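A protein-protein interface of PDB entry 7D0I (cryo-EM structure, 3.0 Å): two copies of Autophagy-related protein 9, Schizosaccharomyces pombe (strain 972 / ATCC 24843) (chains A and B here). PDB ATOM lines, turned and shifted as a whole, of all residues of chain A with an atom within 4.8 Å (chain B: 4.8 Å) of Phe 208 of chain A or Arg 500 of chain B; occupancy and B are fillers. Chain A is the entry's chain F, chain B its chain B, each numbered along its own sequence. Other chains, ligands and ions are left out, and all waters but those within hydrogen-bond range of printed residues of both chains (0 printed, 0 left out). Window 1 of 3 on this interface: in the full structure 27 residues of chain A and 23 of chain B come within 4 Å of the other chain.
The backbone carbonyl oxygen (O) of Phe 208 of chain A sits at hydrogen-bond distance from the side-chain hydroxyl (OG1) of Thr 212 of chain A (2.9 Å).
Phe 208 of chain A touches three residues of chain B. Arg 500 of chain B touches two residues of chain A. Of the printed residues of chain B, Leu 211 of chain A touches Tyr 504 (3.8 Å). Of the printed residues of chain B, Val 204 of chain A touches Asn 497. Met 498 of chain B touches none of the printed residues of chain A. Arg 206 of chain A touches none of the printed residues of chain B. The nearest printed residue of chain B that does not touch Phe 208 of chain A is Asn 497 of chain B (4.8 Å).
Among the printed residues, pairs that only touch across the chains: Val 204 of chain A with Asn 497 of chain B, Phe 208 of chain A with Arg 500 of chain B, Phe 208 of chain A with Leu 501 of chain B, Phe 208 of chain A with Tyr 504 of chain B, Leu 211 of chain A with Tyr 504 of chain B, Thr 212 of chain A with Arg 500 of chain B and Thr 212 of chain A with Tyr 504 of chain B.
No position is printed for both chains.
Printed residues of chain A that touch a printed residue of chain B: Val 204, Phe 208, Leu 211 and Thr 212. Among the printed residues, 7 pairs touch across the chains. Among the printed residues, no Asp or Glu carboxylate lies within 4 Å of a Lys or Arg side-chain nitrogen of the other chain.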
ATOM      1  N   VAL A 204      18.458 -13.046 -23.526  1.00  0.00           N
ATOM      2  CA  VAL A 204      19.455 -13.307 -24.561  1.00  0.00           C
ATOM      3  C   VAL A 204      20.832 -12.842 -24.108  1.00  0.00           C
ATOM      4  O   VAL A 204      21.833 -13.544 -24.297  1.00  0.00           O
ATOM      5  CB  VAL A 204      19.038 -12.644 -25.882  1.00  0.00           C
ATOM      6  CG1 VAL A 204      20.170 -12.697 -26.876  1.00  0.00           C
ATOM      7  CG2 VAL A 204      17.826 -13.338 -26.443  1.00  0.00           C
ATOM      8  N   HIS A 205      20.909 -11.659 -23.499  1.00  0.00           N
ATOM      9  CA  HIS A 205      22.202 -11.150 -23.059  1.00  0.00           C
ATOM     10  C   HIS A 205      22.789 -12.013 -21.956  1.00  0.00           C
ATOM     11  O   HIS A 205      23.982 -12.329 -21.985  1.00  0.00           O
ATOM     12  CB  HIS A 205      22.068  -9.706 -22.591  1.00  0.00           C
ATOM     13  CG  HIS A 205      22.109  -8.707 -23.703  1.00  0.00           C
ATOM     14  ND1 HIS A 205      21.087  -8.568 -24.613  1.00  0.00           N
ATOM     15  CD2 HIS A 205      23.047  -7.793 -24.044  1.00  0.00           C
ATOM     16  CE1 HIS A 205      21.394  -7.614 -25.473  1.00  0.00           C
ATOM     17  NE2 HIS A 205      22.579  -7.129 -25.151  1.00  0.00           N
ATOM     18  N   ARG A 206      21.974 -12.405 -20.978  1.00  0.00           N
ATOM     19  CA  ARG A 206      22.484 -13.261 -19.912  1.00  0.00           C
ATOM     20  C   ARG A 206      22.939 -14.609 -20.457  1.00  0.00           C
ATOM     21  O   ARG A 206      23.972 -15.148 -20.034  1.00  0.00           O
ATOM     22  CB  ARG A 206      21.418 -13.449 -18.840  1.00  0.00           C
ATOM     23  CG  ARG A 206      21.014 -12.169 -18.152  1.00  0.00           C
ATOM     24  CD  ARG A 206      20.022 -12.444 -17.050  1.00  0.00           C
ATOM     25  NE  ARG A 206      19.736 -11.247 -16.276  1.00  0.00           N
ATOM     26  CZ  ARG A 206      18.929 -11.220 -15.225  1.00  0.00           C
ATOM     27  NH1 ARG A 206      18.332 -12.331 -14.820  1.00  0.00           N
ATOM     28  NH2 ARG A 206      18.720 -10.088 -14.576  1.00  0.00           N
ATOM     29  N   LEU A 207      22.179 -15.166 -21.401  1.00  0.00           N
ATOM     30  CA  LEU A 207      22.543 -16.444 -21.996  1.00  0.00           C
ATOM     31  C   LEU A 207      23.876 -16.348 -22.721  1.00  0.00           C
ATOM     32  O   LEU A 207      24.759 -17.186 -22.528  1.00  0.00           O
ATOM     33  CB  LEU A 207      21.444 -16.901 -22.948  1.00  0.00           C
ATOM     34  CG  LEU A 207      21.748 -18.116 -23.812  1.00  0.00           C
ATOM     35  CD1 LEU A 207      22.092 -19.310 -22.947  1.00  0.00           C
ATOM     36  CD2 LEU A 207      20.556 -18.416 -24.696  1.00  0.00           C
ATOM     37  N   PHE A 208      24.043 -15.332 -23.564  1.00  0.00           N
ATOM     38  CA  PHE A 208      25.317 -15.212 -24.258  1.00  0.00           C
ATOM     39  C   PHE A 208      26.452 -14.852 -23.315  1.00  0.00           C
ATOM     40  O   PHE A 208      27.602 -15.170 -23.612  1.00  0.00           O
ATOM     41  CB  PHE A 208      25.219 -14.195 -25.386  1.00  0.00           C
ATOM     42  CG  PHE A 208      24.558 -14.730 -26.615  1.00  0.00           C
ATOM     43  CD1 PHE A 208      25.238 -15.577 -27.459  1.00  0.00           C
ATOM     44  CD2 PHE A 208      23.260 -14.397 -26.918  1.00  0.00           C
ATOM     45  CE1 PHE A 208      24.635 -16.075 -28.581  1.00  0.00           C
ATOM     46  CE2 PHE A 208      22.653 -14.892 -28.041  1.00  0.00           C
ATOM     47  CZ  PHE A 208      23.342 -15.732 -28.874  1.00  0.00           C
ATOM     48  N   GLN A 209      26.154 -14.246 -22.169  1.00  0.00           N
ATOM     49  CA  GLN A 209      27.194 -13.969 -21.188  1.00  0.00           C
ATOM     50  C   GLN A 209      27.720 -15.256 -20.568  1.00  0.00           C
ATOM     51  O   GLN A 209      28.938 -15.482 -20.502  1.00  0.00           O
ATOM     52  CB  GLN A 209      26.643 -13.034 -20.120  1.00  0.00           C
ATOM     53  CG  GLN A 209      27.615 -12.626 -19.048  1.00  0.00           C
ATOM     54  CD  GLN A 209      26.933 -11.814 -17.970  1.00  0.00           C
ATOM     55  OE1 GLN A 209      26.810 -12.255 -16.828  1.00  0.00           O
ATOM     56  NE2 GLN A 209      26.471 -10.625 -18.332  1.00  0.00           N
ATOM     57  N   ILE A 210      26.812 -16.127 -20.116  1.00  0.00           N
ATOM     58  CA  ILE A 210      27.279 -17.398 -19.568  1.00  0.00           C
ATOM     59  C   ILE A 210      27.894 -18.259 -20.661  1.00  0.00           C
ATOM     60  O   ILE A 210      28.828 -19.023 -20.400  1.00  0.00           O
ATOM     61  CB  ILE A 210      26.160 -18.148 -18.826  1.00  0.00           C
ATOM     62  CG1 ILE A 210      24.941 -18.332 -19.718  1.00  0.00           C
ATOM     63  CG2 ILE A 210      25.788 -17.421 -17.555  1.00  0.00           C
ATOM     64  CD1 ILE A 210      23.745 -18.882 -18.995  1.00  0.00           C
ATOM     65  N   LEU A 211      27.419 -18.134 -21.902  1.00  0.00           N
ATOM     66  CA  LEU A 211      28.026 -18.887 -22.994  1.00  0.00           C
ATOM     67  C   LEU A 211      29.446 -18.414 -23.272  1.00  0.00           C
ATOM     68  O   LEU A 211      30.332 -19.230 -23.525  1.00  0.00           O
ATOM     69  CB  LEU A 211      27.173 -18.781 -24.253  1.00  0.00           C
ATOM     70  CG  LEU A 211      25.928 -19.663 -24.300  1.00  0.00           C
ATOM     71  CD1 LEU A 211      25.194 -19.474 -25.608  1.00  0.00           C
ATOM     72  CD2 LEU A 211      26.307 -21.113 -24.104  1.00  0.00           C
ATOM     73  N   THR A 212      29.680 -17.104 -23.226  1.00  0.00           N
ATOM     74  CA  THR A 212      31.027 -16.586 -23.426  1.00  0.00           C
ATOM     75  C   THR A 212      31.959 -17.039 -22.314  1.00  0.00           C
ATOM     76  O   THR A 212      33.095 -17.457 -22.573  1.00  0.00           O
ATOM     77  CB  THR A 212      30.993 -15.064 -23.504  1.00  0.00           C
ATOM     78  OG1 THR A 212      30.238 -14.661 -24.653  1.00  0.00           O
ATOM     79  CG2 THR A 212      32.394 -14.511 -23.607  1.00  0.00           C
ATOM     80  N   PHE B 496      18.753  -6.164 -31.510  1.00  0.00           N
ATOM     81  CA  PHE B 496      19.718  -6.370 -30.438  1.00  0.00           C
ATOM     82  C   PHE B 496      19.945  -7.851 -30.165  1.00  0.00           C
ATOM     83  O   PHE B 496      21.075  -8.268 -29.891  1.00  0.00           O
ATOM     84  CB  PHE B 496      19.255  -5.652 -29.177  1.00  0.00           C
ATOM     85  CG  PHE B 496      19.241  -4.165 -29.310  1.00  0.00           C
ATOM     86  CD1 PHE B 496      20.413  -3.472 -29.538  1.00  0.00           C
ATOM     87  CD2 PHE B 496      18.062  -3.458 -29.199  1.00  0.00           C
ATOM     88  CE1 PHE B 496      20.408  -2.103 -29.660  1.00  0.00           C
ATOM     89  CE2 PHE B 496      18.051  -2.087 -29.320  1.00  0.00           C
ATOM     90  CZ  PHE B 496      19.226  -1.409 -29.550  1.00  0.00           C
ATOM     91  N   ASN B 497      18.891  -8.664 -30.249  1.00  0.00           N
ATOM     92  CA  ASN B 497      19.051 -10.097 -30.047  1.00  0.00           C
ATOM     93  C   ASN B 497      19.873 -10.748 -31.148  1.00  0.00           C
ATOM     94  O   ASN B 497      20.351 -11.870 -30.965  1.00  0.00           O
ATOM     95  CB  ASN B 497      17.687 -10.769 -29.951  1.00  0.00           C
ATOM     96  CG  ASN B 497      16.785 -10.094 -28.951  1.00  0.00           C
ATOM     97  OD1 ASN B 497      16.951  -8.917 -28.652  1.00  0.00           O
ATOM     98  ND2 ASN B 497      15.822 -10.838 -28.425  1.00  0.00           N
ATOM     99  N   MET B 498      20.045 -10.074 -32.282  1.00  0.00           N
ATOM    100  CA  MET B 498      20.895 -10.557 -33.361  1.00  0.00           C
ATOM    101  C   MET B 498      22.286  -9.948 -33.315  1.00  0.00           C
ATOM    102  O   MET B 498      23.271 -10.624 -33.635  1.00  0.00           O
ATOM    103  CB  MET B 498      20.242 -10.255 -34.709  1.00  0.00           C
ATOM    104  CG  MET B 498      20.850 -10.990 -35.881  1.00  0.00           C
ATOM    105  SD  MET B 498      20.045 -10.576 -37.439  1.00  0.00           S
ATOM    106  CE  MET B 498      20.306  -8.802 -37.502  1.00  0.00           C
ATOM    107  N   ILE B 499      22.382  -8.679 -32.917  1.00  0.00           N
ATOM    108  CA  ILE B 499      23.683  -8.070 -32.670  1.00  0.00           C
ATOM    109  C   ILE B 499      24.437  -8.854 -31.611  1.00  0.00           C
ATOM    110  O   ILE B 499      25.645  -9.082 -31.728  1.00  0.00           O
ATOM    111  CB  ILE B 499      23.514  -6.598 -32.256  1.00  0.00           C
ATOM    112  CG1 ILE B 499      22.933  -5.779 -33.400  1.00  0.00           C
ATOM    113  CG2 ILE B 499      24.837  -6.020 -31.820  1.00  0.00           C
ATOM    114  CD1 ILE B 499      22.619  -4.374 -33.005  1.00  0.00           C
ATOM    115  N   ARG B 500      23.734  -9.291 -30.566  1.00  0.00           N
ATOM    116  CA  ARG B 500      24.386 -10.049 -29.506  1.00  0.00           C
ATOM    117  C   ARG B 500      24.895 -11.390 -30.020  1.00  0.00           C
ATOM    118  O   ARG B 500      26.021 -11.799 -29.706  1.00  0.00           O
ATOM    119  CB  ARG B 500      23.415 -10.240 -28.343  1.00  0.00           C
ATOM    120  CG  ARG B 500      24.004 -10.975 -27.176  1.00  0.00           C
ATOM    121  CD  ARG B 500      25.211 -10.255 -26.631  1.00  0.00           C
ATOM    122  NE  ARG B 500      26.209 -11.198 -26.145  1.00  0.00           N
ATOM    123  CZ  ARG B 500      27.390 -10.847 -25.652  1.00  0.00           C
ATOM    124  NH1 ARG B 500      28.238 -11.776 -25.238  1.00  0.00           N
ATOM    125  NH2 ARG B 500      27.721  -9.567 -25.574  1.00  0.00           N
ATOM    126  N   LEU B 501      24.082 -12.084 -30.819  1.00  0.00           N
ATOM    127  CA  LEU B 501      24.510 -13.361 -31.381  1.00  0.00           C
ATOM    128  C   LEU B 501      25.737 -13.194 -32.261  1.00  0.00           C
ATOM    129  O   LEU B 501      26.679 -13.992 -32.187  1.00  0.00           O
ATOM    130  CB  LEU B 501      23.376 -13.990 -32.181  1.00  0.00           C
ATOM    131  CG  LEU B 501      23.816 -15.111 -33.119  1.00  0.00           C
ATOM    132  CD1 LEU B 501      24.223 -16.334 -32.331  1.00  0.00           C
ATOM    133  CD2 LEU B 501      22.718 -15.444 -34.100  1.00  0.00           C
ATOM    134  N   PHE B 502      25.742 -12.173 -33.114  1.00  0.00           N
ATOM    135  CA  PHE B 502      26.890 -11.999 -33.991  1.00  0.00           C
ATOM    136  C   PHE B 502      28.119 -11.548 -33.220  1.00  0.00           C
ATOM    137  O   PHE B 502      29.240 -11.896 -33.597  1.00  0.00           O
ATOM    138  CB  PHE B 502      26.553 -11.029 -35.115  1.00  0.00           C
ATOM    139  CG  PHE B 502      25.767 -11.659 -36.220  1.00  0.00           C
ATOM    140  CD1 PHE B 502      26.339 -12.631 -37.019  1.00  0.00           C
ATOM    141  CD2 PHE B 502      24.456 -11.299 -36.452  1.00  0.00           C
ATOM    142  CE1 PHE B 502      25.625 -13.225 -38.026  1.00  0.00           C
ATOM    143  CE2 PHE B 502      23.737 -11.889 -37.462  1.00  0.00           C
ATOM    144  CZ  PHE B 502      24.321 -12.853 -38.251  1.00  0.00           C
ATOM    145  N   LYS B 503      27.934 -10.801 -32.130  1.00  0.00           N
ATOM    146  CA  LYS B 503      29.059 -10.486 -31.256  1.00  0.00           C
ATOM    147  C   LYS B 503      29.657 -11.756 -30.670  1.00  0.00           C
ATOM    148  O   LYS B 503      30.882 -11.922 -30.638  1.00  0.00           O
ATOM    149  CB  LYS B 503      28.598  -9.543 -30.144  1.00  0.00           C
ATOM    150  CG  LYS B 503      29.692  -8.699 -29.532  1.00  0.00           C
ATOM    151  CD  LYS B 503      29.231  -8.068 -28.225  1.00  0.00           C
ATOM    152  CE  LYS B 503      27.996  -7.206 -28.414  1.00  0.00           C
ATOM    153  NZ  LYS B 503      27.420  -6.771 -27.108  1.00  0.00           N
ATOM    154  N   TYR B 504      28.801 -12.677 -30.229  1.00  0.00           N
ATOM    155  CA  TYR B 504      29.283 -13.946 -29.690  1.00  0.00           C
ATOM    156  C   TYR B 504      30.034 -14.751 -30.744  1.00  0.00           C
ATOM    157  O   TYR B 504      31.101 -15.319 -30.469  1.00  0.00           O
ATOM    158  CB  TYR B 504      28.109 -14.747 -29.143  1.00  0.00           C
ATOM    159  CG  TYR B 504      28.486 -16.111 -28.641  1.00  0.00           C
ATOM    160  CD1 TYR B 504      29.555 -16.280 -27.783  1.00  0.00           C
ATOM    161  CD2 TYR B 504      27.761 -17.227 -29.010  1.00  0.00           C
ATOM    162  CE1 TYR B 504      29.899 -17.523 -27.315  1.00  0.00           C
ATOM    163  CE2 TYR B 504      28.097 -18.474 -28.545  1.00  0.00           C
ATOM    164  CZ  TYR B 504      29.168 -18.616 -27.698  1.00  0.00           C
ATOM    165  OH  TYR B 504      29.512 -19.857 -27.229  1.00  0.00           O
